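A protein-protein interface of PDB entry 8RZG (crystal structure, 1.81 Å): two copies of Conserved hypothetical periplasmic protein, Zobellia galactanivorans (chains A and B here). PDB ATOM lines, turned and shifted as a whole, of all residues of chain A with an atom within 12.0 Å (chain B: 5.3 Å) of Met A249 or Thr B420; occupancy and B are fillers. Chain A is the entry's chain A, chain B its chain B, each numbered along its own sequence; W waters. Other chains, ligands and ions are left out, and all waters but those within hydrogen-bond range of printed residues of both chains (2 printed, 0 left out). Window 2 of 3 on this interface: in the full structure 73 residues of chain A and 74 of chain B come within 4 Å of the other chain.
Of the 23 printed residues of chain A, 6 touch a printed residue of chain B.
Hydrophobic or aromatic side chains of chain A that line the printed part of chain B: Tyr A188 and Met A249.
Printed residues of chain B within 4 Å of Tyr A188: Glu B413 (3.7 Å).
Of the printed residues of chain B, Gly A247 touches Leu B431 (3.1 Å).
Printed residues of chain B within 4 Å of Val A248: Thr B434 (3.9 Å).
Of the printed residues of chain B, Met A249 touches Phe B418 (3.6 Å), Thr B420 (3.998 Å), Thr B434 (3.9 Å) and Arg B440 (3.8 Å).
Phe B418 touches just one residue of chain A: Met A249.
No residue of chain A comes within 4 Å of Thr B419.
Of the printed residues of chain A, Thr B420 touches Met A249 (3.998 Å).
No residue of chain A comes within 4 Å of Asp B421.
No residue of chain A comes within 4 Å of Leu B422.
No residue of chain A comes within 4 Å of Met B423.
The nearest printed residue of chain B that does not touch Asn A244 is Leu B431 (5.2 Å).
Water W2 lies within hydrogen-bond range of the backbone carbonyl oxygen of Gly A247 and the guanidinium group of Arg B425.
Water W1 lies within hydrogen-bond range of the side-chain amide nitrogen of Asn A238 (2.8 Å), the side-chain carboxylate of Glu B413 (2.8 Å) and the side-chain amide oxygen of Gln A240 (2.8 Å).
The side-chain hydroxyl (OG1) of Thr B434 is in hydrogen-bond range of the side-chain amide oxygen (OD1) of Asn A244, at 2.8 Å.
The backbone NH of Leu B431 lies within hydrogen-bond range of the backbone carbonyl oxygen of Gly A247 (3.1 Å).
NE2 of Gln A240 sits at hydrogen-bond distance from O of Val A248 (2.9 Å).
The backbone NH (N) of Gln A240 sits at hydrogen-bond distance from the side-chain amide oxygen (OD1) of Asn A237, 3.4 Å away.
The backbone carbonyl oxygen (O) of Phe A243 lies within hydrogen-bond range of the backbone NH (N) of Val A248 (3.4 Å).
The side-chain amide oxygen of Gln A240 is in hydrogen-bond range of the backbone NH of Ser A250 (2.8 Å).
NE2 of Gln A240 lies within hydrogen-bond range of OD1 of Asn A244 (3.1 Å).
OD1 of Asn A238 lies within hydrogen-bond range of N of Gln A240.
No position is printed for both chains.
CE1 of Tyr A188 touches OE1 of Glu B413, 3.7 Å away.
O of Thr B434 touches CG of Gln A240 (3.5 Å).
Thr B434 touches Val A248.
CE of Met A249 touches CZ of Phe B418, at 3.6 Å.
Thr B420 touches Met A249 (CG2 to CG, 3.998 Å).
SD of Met A249 touches CG2 of Thr B434 (3.9 Å).
Met A249 touches Arg B440.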
ATOM      1  N   TRP A  53      13.864 -32.689  -2.370  1.00  0.00           N
ATOM      2  CA  TRP A  53      14.833 -32.545  -1.286  1.00  0.00           C
ATOM      3  C   TRP A  53      14.793 -33.707  -0.291  1.00  0.00           C
ATOM      4  O   TRP A  53      15.826 -34.321  -0.008  1.00  0.00           O
ATOM      5  CB  TRP A  53      14.600 -31.231  -0.539  1.00  0.00           C
ATOM      6  CG  TRP A  53      14.909 -29.991  -1.322  1.00  0.00           C
ATOM      7  CD1 TRP A  53      15.478 -29.917  -2.562  1.00  0.00           C
ATOM      8  CD2 TRP A  53      14.665 -28.642  -0.907  1.00  0.00           C
ATOM      9  NE1 TRP A  53      15.607 -28.596  -2.945  1.00  0.00           N
ATOM     10  CE2 TRP A  53      15.116 -27.796  -1.944  1.00  0.00           C
ATOM     11  CE3 TRP A  53      14.120 -28.066   0.246  1.00  0.00           C
ATOM     12  CZ2 TRP A  53      15.022 -26.410  -1.867  1.00  0.00           C
ATOM     13  CZ3 TRP A  53      14.024 -26.684   0.319  1.00  0.00           C
ATOM     14  CH2 TRP A  53      14.475 -25.874  -0.729  1.00  0.00           C
ATOM     15  N   GLU A  54      13.619 -33.990   0.275  1.00  0.00           N
ATOM     16  CA  GLU A  54      13.496 -34.937   1.380  1.00  0.00           C
ATOM     17  C   GLU A  54      12.490 -36.052   1.121  1.00  0.00           C
ATOM     18  O   GLU A  54      12.226 -36.850   2.030  1.00  0.00           O
ATOM     19  CB  GLU A  54      13.106 -34.209   2.671  1.00  0.00           C
ATOM     20  CG  GLU A  54      14.183 -33.315   3.246  1.00  0.00           C
ATOM     21  CD  GLU A  54      13.648 -32.335   4.282  1.00  0.00           C
ATOM     22  OE1 GLU A  54      12.478 -32.482   4.701  1.00  0.00           O
ATOM     23  OE2 GLU A  54      14.400 -31.413   4.673  1.00  0.00           O
ATOM     24  N   THR A 187      18.474 -15.275  -4.618  1.00  0.00           N
ATOM     25  CA  THR A 187      18.221 -16.713  -4.715  1.00  0.00           C
ATOM     26  C   THR A 187      19.101 -17.538  -3.786  1.00  0.00           C
ATOM     27  O   THR A 187      18.892 -18.757  -3.687  1.00  0.00           O
ATOM     28  CB  THR A 187      18.423 -17.221  -6.143  1.00  0.00           C
ATOM     29  OG1 THR A 187      19.823 -17.224  -6.458  1.00  0.00           O
ATOM     30  CG2 THR A 187      17.679 -16.350  -7.129  1.00  0.00           C
ATOM     31  N   TYR A 188      20.082 -16.925  -3.123  1.00  0.00           N
ATOM     32  CA  TYR A 188      20.941 -17.626  -2.174  1.00  0.00           C
ATOM     33  C   TYR A 188      20.716 -17.184  -0.738  1.00  0.00           C
ATOM     34  O   TYR A 188      21.381 -17.702   0.161  1.00  0.00           O
ATOM     35  CB  TYR A 188      22.424 -17.444  -2.533  1.00  0.00           C
ATOM     36  CG  TYR A 188      22.907 -18.339  -3.663  1.00  0.00           C
ATOM     37  CD1 TYR A 188      23.202 -19.681  -3.439  1.00  0.00           C
ATOM     38  CD2 TYR A 188      23.074 -17.834  -4.945  1.00  0.00           C
ATOM     39  CE1 TYR A 188      23.644 -20.499  -4.472  1.00  0.00           C
ATOM     40  CE2 TYR A 188      23.513 -18.637  -5.978  1.00  0.00           C
ATOM     41  CZ  TYR A 188      23.803 -19.966  -5.740  1.00  0.00           C
ATOM     42  OH  TYR A 188      24.240 -20.755  -6.778  1.00  0.00           O
ATOM     43  N   ASN A 189      19.819 -16.233  -0.494  1.00  0.00           N
ATOM     44  CA  ASN A 189      19.524 -15.874   0.886  1.00  0.00           C
ATOM     45  C   ASN A 189      18.026 -15.881   1.130  1.00  0.00           C
ATOM     46  O   ASN A 189      17.254 -16.371   0.298  1.00  0.00           O
ATOM     47  CB  ASN A 189      20.153 -14.518   1.261  1.00  0.00           C
ATOM     48  CG  ASN A 189      19.632 -13.353   0.431  1.00  0.00           C
ATOM     49  OD1 ASN A 189      18.476 -13.329  -0.001  1.00  0.00           O
ATOM     50  ND2 ASN A 189      20.493 -12.354   0.230  1.00  0.00           N
ATOM     51  N   ASN A 237      16.033 -21.134  -4.569  1.00  0.00           N
ATOM     52  CA  ASN A 237      16.798 -21.328  -3.350  1.00  0.00           C
ATOM     53  C   ASN A 237      17.044 -22.821  -3.135  1.00  0.00           C
ATOM     54  O   ASN A 237      16.168 -23.647  -3.413  1.00  0.00           O
ATOM     55  CB  ASN A 237      16.029 -20.723  -2.171  1.00  0.00           C
ATOM     56  CG  ASN A 237      16.870 -20.576  -0.913  1.00  0.00           C
ATOM     57  OD1 ASN A 237      17.408 -21.549  -0.380  1.00  0.00           O
ATOM     58  ND2 ASN A 237      16.957 -19.348  -0.412  1.00  0.00           N
ATOM     59  N   ASN A 238      18.243 -23.167  -2.661  1.00  0.00           N
ATOM     60  CA  ASN A 238      18.589 -24.570  -2.430  1.00  0.00           C
ATOM     61  C   ASN A 238      18.209 -25.057  -1.040  1.00  0.00           C
ATOM     62  O   ASN A 238      18.616 -26.160  -0.654  1.00  0.00           O
ATOM     63  CB  ASN A 238      20.088 -24.806  -2.656  1.00  0.00           C
ATOM     64  CG  ASN A 238      20.972 -24.060  -1.653  1.00  0.00           C
ATOM     65  OD1 ASN A 238      20.489 -23.443  -0.694  1.00  0.00           O
ATOM     66  ND2 ASN A 238      22.280 -24.126  -1.870  1.00  0.00           N
ATOM     67  N   GLY A 239      17.468 -24.259  -0.275  1.00  0.00           N
ATOM     68  CA  GLY A 239      17.089 -24.656   1.071  1.00  0.00           C
ATOM     69  C   GLY A 239      18.113 -24.363   2.144  1.00  0.00           C
ATOM     70  O   GLY A 239      18.029 -24.936   3.237  1.00  0.00           O
ATOM     71  N   GLN A 240      19.085 -23.485   1.870  1.00  0.00           N
ATOM     72  CA  GLN A 240      20.093 -23.154   2.874  1.00  0.00           C
ATOM     73  C   GLN A 240      19.449 -22.600   4.140  1.00  0.00           C
ATOM     74  O   GLN A 240      19.997 -22.762   5.240  1.00  0.00           O
ATOM     75  CB  GLN A 240      21.106 -22.157   2.291  1.00  0.00           C
ATOM     76  CG  GLN A 240      22.274 -21.816   3.214  1.00  0.00           C
ATOM     77  CD  GLN A 240      23.054 -23.040   3.648  1.00  0.00           C
ATOM     78  OE1 GLN A 240      23.530 -23.817   2.816  1.00  0.00           O
ATOM     79  NE2 GLN A 240      23.185 -23.227   4.958  1.00  0.00           N
ATOM     80  N   TYR A 241      18.275 -21.975   4.014  1.00  0.00           N
ATOM     81  CA  TYR A 241      17.577 -21.453   5.187  1.00  0.00           C
ATOM     82  C   TYR A 241      17.186 -22.549   6.175  1.00  0.00           C
ATOM     83  O   TYR A 241      16.949 -22.249   7.352  1.00  0.00           O
ATOM     84  CB  TYR A 241      16.337 -20.663   4.764  1.00  0.00           C
ATOM     85  CG  TYR A 241      15.374 -21.409   3.865  1.00  0.00           C
ATOM     86  CD1 TYR A 241      15.556 -21.426   2.486  1.00  0.00           C
ATOM     87  CD2 TYR A 241      14.273 -22.078   4.390  1.00  0.00           C
ATOM     88  CE1 TYR A 241      14.680 -22.096   1.658  1.00  0.00           C
ATOM     89  CE2 TYR A 241      13.380 -22.754   3.563  1.00  0.00           C
ATOM     90  CZ  TYR A 241      13.593 -22.756   2.197  1.00  0.00           C
ATOM     91  OH  TYR A 241      12.731 -23.419   1.358  1.00  0.00           O
ATOM     92  N   LEU A 242      17.116 -23.806   5.733  1.00  0.00           N
ATOM     93  CA  LEU A 242      16.811 -24.896   6.653  1.00  0.00           C
ATOM     94  C   LEU A 242      18.012 -25.326   7.486  1.00  0.00           C
ATOM     95  O   LEU A 242      17.832 -26.044   8.476  1.00  0.00           O
ATOM     96  CB  LEU A 242      16.274 -26.108   5.879  1.00  0.00           C
ATOM     97  CG  LEU A 242      15.026 -25.864   5.024  1.00  0.00           C
ATOM     98  CD1 LEU A 242      14.785 -27.050   4.098  1.00  0.00           C
ATOM     99  CD2 LEU A 242      13.802 -25.599   5.904  1.00  0.00           C
ATOM    100  N   PHE A 243      19.221 -24.905   7.115  1.00  0.00           N
ATOM    101  CA  PHE A 243      20.444 -25.398   7.728  1.00  0.00           C
ATOM    102  C   PHE A 243      21.285 -24.314   8.384  1.00  0.00           C
ATOM    103  O   PHE A 243      22.303 -24.642   9.006  1.00  0.00           O
ATOM    104  CB  PHE A 243      21.295 -26.129   6.679  1.00  0.00           C
ATOM    105  CG  PHE A 243      20.598 -27.301   6.055  1.00  0.00           C
ATOM    106  CD1 PHE A 243      20.697 -28.557   6.624  1.00  0.00           C
ATOM    107  CD2 PHE A 243      19.830 -27.142   4.913  1.00  0.00           C
ATOM    108  CE1 PHE A 243      20.051 -29.642   6.062  1.00  0.00           C
ATOM    109  CE2 PHE A 243      19.182 -28.228   4.340  1.00  0.00           C
ATOM    110  CZ  PHE A 243      19.289 -29.474   4.918  1.00  0.00           C
ATOM    111  N   ASN A 244      20.895 -23.041   8.265  1.00  0.00           N
ATOM    112  CA  ASN A 244      21.703 -21.966   8.829  1.00  0.00           C
ATOM    113  C   ASN A 244      21.833 -22.102  10.341  1.00  0.00           C
ATOM    114  O   ASN A 244      22.931 -21.950  10.893  1.00  0.00           O
ATOM    115  CB  ASN A 244      21.105 -20.607   8.456  1.00  0.00           C
ATOM    116  CG  ASN A 244      21.362 -20.235   7.004  1.00  0.00           C
ATOM    117  OD1 ASN A 244      22.345 -20.668   6.410  1.00  0.00           O
ATOM    118  ND2 ASN A 244      20.474 -19.428   6.429  1.00  0.00           N
ATOM    119  N   ALA A 245      20.726 -22.396  11.032  1.00  0.00           N
ATOM    120  CA  ALA A 245      20.793 -22.528  12.485  1.00  0.00           C
ATOM    121  C   ALA A 245      21.702 -23.679  12.903  1.00  0.00           C
ATOM    122  O   ALA A 245      22.347 -23.612  13.956  1.00  0.00           O
ATOM    123  CB  ALA A 245      19.385 -22.714  13.063  1.00  0.00           C
ATOM    124  N   LYS A 246      21.777 -24.733  12.091  1.00  0.00           N
ATOM    125  CA  LYS A 246      22.689 -25.837  12.358  1.00  0.00           C
ATOM    126  C   LYS A 246      24.118 -25.542  11.918  1.00  0.00           C
ATOM    127  O   LYS A 246      25.030 -26.288  12.291  1.00  0.00           O
ATOM    128  CB  LYS A 246      22.198 -27.105  11.657  1.00  0.00           C
ATOM    129  CG  LYS A 246      20.848 -27.617  12.134  1.00  0.00           C
ATOM    130  CD  LYS A 246      20.248 -28.557  11.095  1.00  0.00           C
ATOM    131  CE  LYS A 246      19.125 -29.402  11.670  1.00  0.00           C
ATOM    132  NZ  LYS A 246      18.621 -30.371  10.656  1.00  0.00           N
ATOM    133  N   GLY A 247      24.332 -24.488  11.138  1.00  0.00           N
ATOM    134  CA  GLY A 247      25.669 -24.160  10.679  1.00  0.00           C
ATOM    135  C   GLY A 247      26.287 -25.189   9.758  1.00  0.00           C
ATOM    136  O   GLY A 247      27.476 -25.498   9.896  1.00  0.00           O
ATOM    137  N   VAL A 248      25.506 -25.748   8.831  1.00  0.00           N
ATOM    138  CA  VAL A 248      26.029 -26.638   7.805  1.00  0.00           C
ATOM    139  C   VAL A 248      25.533 -26.157   6.446  1.00  0.00           C
ATOM    140  O   VAL A 248      24.622 -25.331   6.342  1.00  0.00           O
ATOM    141  CB  VAL A 248      25.631 -28.117   8.034  1.00  0.00           C
ATOM    142  CG1 VAL A 248      25.961 -28.556   9.457  1.00  0.00           C
ATOM    143  CG2 VAL A 248      24.157 -28.330   7.726  1.00  0.00           C
ATOM    144  N   MET A 249      26.164 -26.675   5.398  1.00  0.00           N
ATOM    145  CA  MET A 249      25.809 -26.320   4.030  1.00  0.00           C
ATOM    146  C   MET A 249      24.651 -27.184   3.551  1.00  0.00           C
ATOM    147  O   MET A 249      24.594 -28.381   3.847  1.00  0.00           O
ATOM    148  CB  MET A 249      27.020 -26.499   3.106  1.00  0.00           C
ATOM    149  CG  MET A 249      28.240 -25.669   3.492  1.00  0.00           C
ATOM    150  SD  MET A 249      27.835 -23.897   3.529  1.00  0.00           S
ATOM    151  CE  MET A 249      27.426 -23.582   1.821  1.00  0.00           C
ATOM    152  N   SER A 250      23.723 -26.580   2.818  1.00  0.00           N
ATOM    153  CA  SER A 250      22.588 -27.335   2.299  1.00  0.00           C
ATOM    154  C   SER A 250      23.065 -28.394   1.306  1.00  0.00           C
ATOM    155  O   SER A 250      23.898 -28.096   0.441  1.00  0.00           O
ATOM    156  CB  SER A 250      21.580 -26.411   1.618  1.00  0.00           C
ATOM    157  OG  SER A 250      20.585 -27.174   0.945  1.00  0.00           O
ATOM    158  N   PRO A 251      22.565 -29.627   1.391  1.00  0.00           N
ATOM    159  CA  PRO A 251      22.866 -30.641   0.374  1.00  0.00           C
ATOM    160  C   PRO A 251      21.887 -30.690  -0.787  1.00  0.00           C
ATOM    161  O   PRO A 251      22.002 -31.598  -1.619  1.00  0.00           O
ATOM    162  CB  PRO A 251      22.783 -31.941   1.188  1.00  0.00           C
ATOM    163  CG  PRO A 251      21.630 -31.672   2.113  1.00  0.00           C
ATOM    164  CD  PRO A 251      21.735 -30.186   2.478  1.00  0.00           C
ATOM    165  N   TYR A 252      20.935 -29.762  -0.862  1.00  0.00           N
ATOM    166  CA  TYR A 252      19.838 -29.820  -1.815  1.00  0.00           C
ATOM    167  C   TYR A 252      20.139 -29.012  -3.070  1.00  0.00           C
ATOM    168  O   TYR A 252      21.048 -28.180  -3.109  1.00  0.00           O
ATOM    169  CB  TYR A 252      18.545 -29.303  -1.185  1.00  0.00           C
ATOM    170  CG  TYR A 252      18.128 -30.027   0.068  1.00  0.00           C
ATOM    171  CD1 TYR A 252      18.409 -31.379   0.243  1.00  0.00           C
ATOM    172  CD2 TYR A 252      17.449 -29.362   1.078  1.00  0.00           C
ATOM    173  CE1 TYR A 252      18.025 -32.042   1.402  1.00  0.00           C
ATOM    174  CE2 TYR A 252      17.068 -30.010   2.232  1.00  0.00           C
ATOM    175  CZ  TYR A 252      17.354 -31.347   2.390  1.00  0.00           C
ATOM    176  OH  TYR A 252      16.967 -31.983   3.543  1.00  0.00           O
ATOM    177  N   GLN A 253      19.329 -29.245  -4.098  1.00  0.00           N
ATOM    178  CA  GLN A 253      19.460 -28.538  -5.363  1.00  0.00           C
ATOM    179  C   GLN A 253      18.578 -27.297  -5.396  1.00  0.00           C
ATOM    180  O   GLN A 253      17.488 -27.268  -4.819  1.00  0.00           O
ATOM    181  CB  GLN A 253      19.094 -29.447  -6.539  1.00  0.00           C
ATOM    182  N   ARG A 254      19.062 -26.275  -6.096  1.00  0.00           N
ATOM    183  CA  ARG A 254      18.280 -25.071  -6.340  1.00  0.00           C
ATOM    184  C   ARG A 254      17.039 -25.405  -7.159  1.00  0.00           C
ATOM    185  O   ARG A 254      17.142 -25.951  -8.262  1.00  0.00           O
ATOM    186  CB  ARG A 254      19.147 -24.039  -7.068  1.00  0.00           C
ATOM    187  CG  ARG A 254      20.176 -23.393  -6.165  1.00  0.00           C
ATOM    188  CD  ARG A 254      21.331 -22.742  -6.926  1.00  0.00           C
ATOM    189  NE  ARG A 254      20.953 -21.666  -7.846  1.00  0.00           N
ATOM    190  CZ  ARG A 254      20.636 -20.428  -7.473  1.00  0.00           C
ATOM    191  NH1 ARG A 254      20.352 -19.513  -8.395  1.00  0.00           N
ATOM    192  NH2 ARG A 254      20.593 -20.096  -6.181  1.00  0.00           N
ATOM    193  N   GLU B 413      28.929 -21.757  -3.732  1.00  0.00           N
ATOM    194  CA  GLU B 413      28.398 -23.103  -3.926  1.00  0.00           C
ATOM    195  C   GLU B 413      28.610 -23.611  -5.341  1.00  0.00           C
ATOM    196  O   GLU B 413      28.731 -24.823  -5.545  1.00  0.00           O
ATOM    197  CB  GLU B 413      26.899 -23.141  -3.621  1.00  0.00           C
ATOM    198  CG  GLU B 413      26.525 -22.954  -2.166  1.00  0.00           C
ATOM    199  CD  GLU B 413      26.251 -21.512  -1.816  1.00  0.00           C
ATOM    200  OE1 GLU B 413      26.768 -20.626  -2.514  1.00  0.00           O
ATOM    201  OE2 GLU B 413      25.518 -21.263  -0.835  1.00  0.00           O
ATOM    202  N   PHE B 418      34.893 -25.153  -4.261  1.00  0.00           N
ATOM    203  CA  PHE B 418      34.257 -24.851  -2.982  1.00  0.00           C
ATOM    204  C   PHE B 418      34.741 -25.810  -1.903  1.00  0.00           C
ATOM    205  O   PHE B 418      34.842 -27.019  -2.120  1.00  0.00           O
ATOM    206  CB  PHE B 418      32.732 -24.941  -3.093  1.00  0.00           C
ATOM    207  CG  PHE B 418      32.017 -24.791  -1.763  1.00  0.00           C
ATOM    208  CD1 PHE B 418      31.764 -25.893  -0.955  1.00  0.00           C
ATOM    209  CD2 PHE B 418      31.606 -23.551  -1.329  1.00  0.00           C
ATOM    210  CE1 PHE B 418      31.121 -25.749   0.264  1.00  0.00           C
ATOM    211  CE2 PHE B 418      30.952 -23.397  -0.115  1.00  0.00           C
ATOM    212  CZ  PHE B 418      30.716 -24.500   0.686  1.00  0.00           C
ATOM    213  N   THR B 419      35.023 -25.261  -0.727  1.00  0.00           N
ATOM    214  CA  THR B 419      35.414 -26.044   0.433  1.00  0.00           C
ATOM    215  C   THR B 419      35.018 -25.263   1.675  1.00  0.00           C
ATOM    216  O   THR B 419      35.036 -24.032   1.679  1.00  0.00           O
ATOM    217  CB  THR B 419      36.925 -26.341   0.442  1.00  0.00           C
ATOM    218  OG1 THR B 419      37.296 -26.949   1.683  1.00  0.00           O
ATOM    219  CG2 THR B 419      37.733 -25.058   0.265  1.00  0.00           C
ATOM    220  N   THR B 420      34.647 -25.984   2.724  1.00  0.00           N
ATOM    221  CA  THR B 420      34.438 -25.331   4.009  1.00  0.00           C
ATOM    222  C   THR B 420      35.737 -25.156   4.795  1.00  0.00           C
ATOM    223  O   THR B 420      35.706 -24.576   5.887  1.00  0.00           O
ATOM    224  CB  THR B 420      33.422 -26.129   4.828  1.00  0.00           C
ATOM    225  OG1 THR B 420      33.965 -27.416   5.116  1.00  0.00           O
ATOM    226  CG2 THR B 420      32.148 -26.318   4.030  1.00  0.00           C
ATOM    227  N   ASP B 421      36.869 -25.625   4.253  1.00  0.00           N
ATOM    228  CA  ASP B 421      38.152 -25.528   4.948  1.00  0.00           C
ATOM    229  C   ASP B 421      38.517 -24.085   5.279  1.00  0.00           C
ATOM    230  O   ASP B 421      39.100 -23.814   6.334  1.00  0.00           O
ATOM    231  CB  ASP B 421      39.261 -26.155   4.107  1.00  0.00           C
ATOM    232  CG  ASP B 421      39.141 -27.658   4.017  1.00  0.00           C
ATOM    233  OD1 ASP B 421      38.313 -28.236   4.754  1.00  0.00           O
ATOM    234  OD2 ASP B 421      39.874 -28.264   3.203  1.00  0.00           O
ATOM    235  N   LEU B 422      38.213 -23.149   4.384  1.00  0.00           N
ATOM    236  CA  LEU B 422      38.567 -21.750   4.598  1.00  0.00           C
ATOM    237  C   LEU B 422      37.498 -20.972   5.352  1.00  0.00           C
ATOM    238  O   LEU B 422      37.644 -19.758   5.533  1.00  0.00           O
ATOM    239  CB  LEU B 422      38.862 -21.068   3.256  1.00  0.00           C
ATOM    240  CG  LEU B 422      40.113 -21.569   2.519  1.00  0.00           C
ATOM    241  CD1 LEU B 422      40.192 -21.030   1.101  1.00  0.00           C
ATOM    242  CD2 LEU B 422      41.368 -21.202   3.268  1.00  0.00           C
ATOM    243  N   MET B 423      36.430 -21.629   5.795  1.00  0.00           N
ATOM    244  CA  MET B 423      35.360 -20.917   6.479  1.00  0.00           C
ATOM    245  C   MET B 423      35.624 -20.889   7.982  1.00  0.00           C
ATOM    246  O   MET B 423      36.438 -21.646   8.511  1.00  0.00           O
ATOM    247  CB  MET B 423      33.994 -21.553   6.175  1.00  0.00           C
ATOM    248  CG  MET B 423      33.536 -21.390   4.709  1.00  0.00           C
ATOM    249  SD  MET B 423      31.948 -22.154   4.249  1.00  0.00           S
ATOM    250  CE  MET B 423      30.818 -21.240   5.284  1.00  0.00           C
ATOM    251  N   ARG B 425      34.330 -21.057  12.026  1.00  0.00           N
ATOM    252  CA  ARG B 425      33.382 -21.729  12.899  1.00  0.00           C
ATOM    253  C   ARG B 425      33.254 -20.965  14.211  1.00  0.00           C
ATOM    254  O   ARG B 425      34.179 -20.268  14.632  1.00  0.00           O
ATOM    255  CB  ARG B 425      33.804 -23.173  13.161  1.00  0.00           C
ATOM    256  CG  ARG B 425      33.789 -24.020  11.895  1.00  0.00           C
ATOM    257  CD  ARG B 425      34.283 -25.440  12.125  1.00  0.00           C
ATOM    258  NE  ARG B 425      34.286 -26.179  10.867  1.00  0.00           N
ATOM    259  CZ  ARG B 425      33.260 -26.903  10.427  1.00  0.00           C
ATOM    260  NH1 ARG B 425      32.155 -26.995  11.156  1.00  0.00           N
ATOM    261  NH2 ARG B 425      33.346 -27.546   9.266  1.00  0.00           N
ATOM    262  N   LEU B 431      29.642 -23.799  11.292  1.00  0.00           N
ATOM    263  CA  LEU B 431      30.076 -22.874  10.256  1.00  0.00           C
ATOM    264  C   LEU B 431      29.347 -21.546  10.384  1.00  0.00           C
ATOM    265  O   LEU B 431      28.138 -21.497  10.639  1.00  0.00           O
ATOM    266  CB  LEU B 431      29.822 -23.467   8.872  1.00  0.00           C
ATOM    267  CG  LEU B 431      30.702 -24.631   8.428  1.00  0.00           C
ATOM    268  CD1 LEU B 431      30.191 -25.186   7.109  1.00  0.00           C
ATOM    269  CD2 LEU B 431      32.145 -24.163   8.289  1.00  0.00           C
ATOM    270  N   THR B 434      26.992 -19.266   6.690  1.00  0.00           N
ATOM    271  CA  THR B 434      26.413 -20.177   5.709  1.00  0.00           C
ATOM    272  C   THR B 434      25.356 -19.487   4.861  1.00  0.00           C
ATOM    273  O   THR B 434      25.131 -19.892   3.715  1.00  0.00           O
ATOM    274  CB  THR B 434      25.823 -21.411   6.394  1.00  0.00           C
ATOM    275  OG1 THR B 434      24.915 -21.008   7.426  1.00  0.00           O
ATOM    276  CG2 THR B 434      26.935 -22.265   6.993  1.00  0.00           C
ATOM    277  N   ARG B 440      32.375 -15.508   3.303  1.00  0.00           N
ATOM    278  CA  ARG B 440      32.536 -16.779   3.996  1.00  0.00           C
ATOM    279  C   ARG B 440      33.975 -17.119   4.363  1.00  0.00           C
ATOM    280  O   ARG B 440      34.181 -17.921   5.281  1.00  0.00           O
ATOM    281  CB  ARG B 440      31.969 -17.928   3.145  1.00  0.00           C
ATOM    282  CG  ARG B 440      30.462 -18.101   3.238  1.00  0.00           C
ATOM    283  CD  ARG B 440      29.972 -19.162   2.262  1.00  0.00           C
ATOM    284  NE  ARG B 440      28.521 -19.330   2.314  1.00  0.00           N
ATOM    285  CZ  ARG B 440      27.795 -19.839   1.323  1.00  0.00           C
ATOM    286  NH1 ARG B 440      26.477 -19.952   1.450  1.00  0.00           N
ATOM    287  NH2 ARG B 440      28.384 -20.220   0.195  1.00  0.00           N
HETATM  288  O   HOH W   1      24.105 -23.456   0.097  1.00  0.00           O
HETATM  289  O   HOH W   2      29.173 -27.382  10.603  1.00  0.00           O
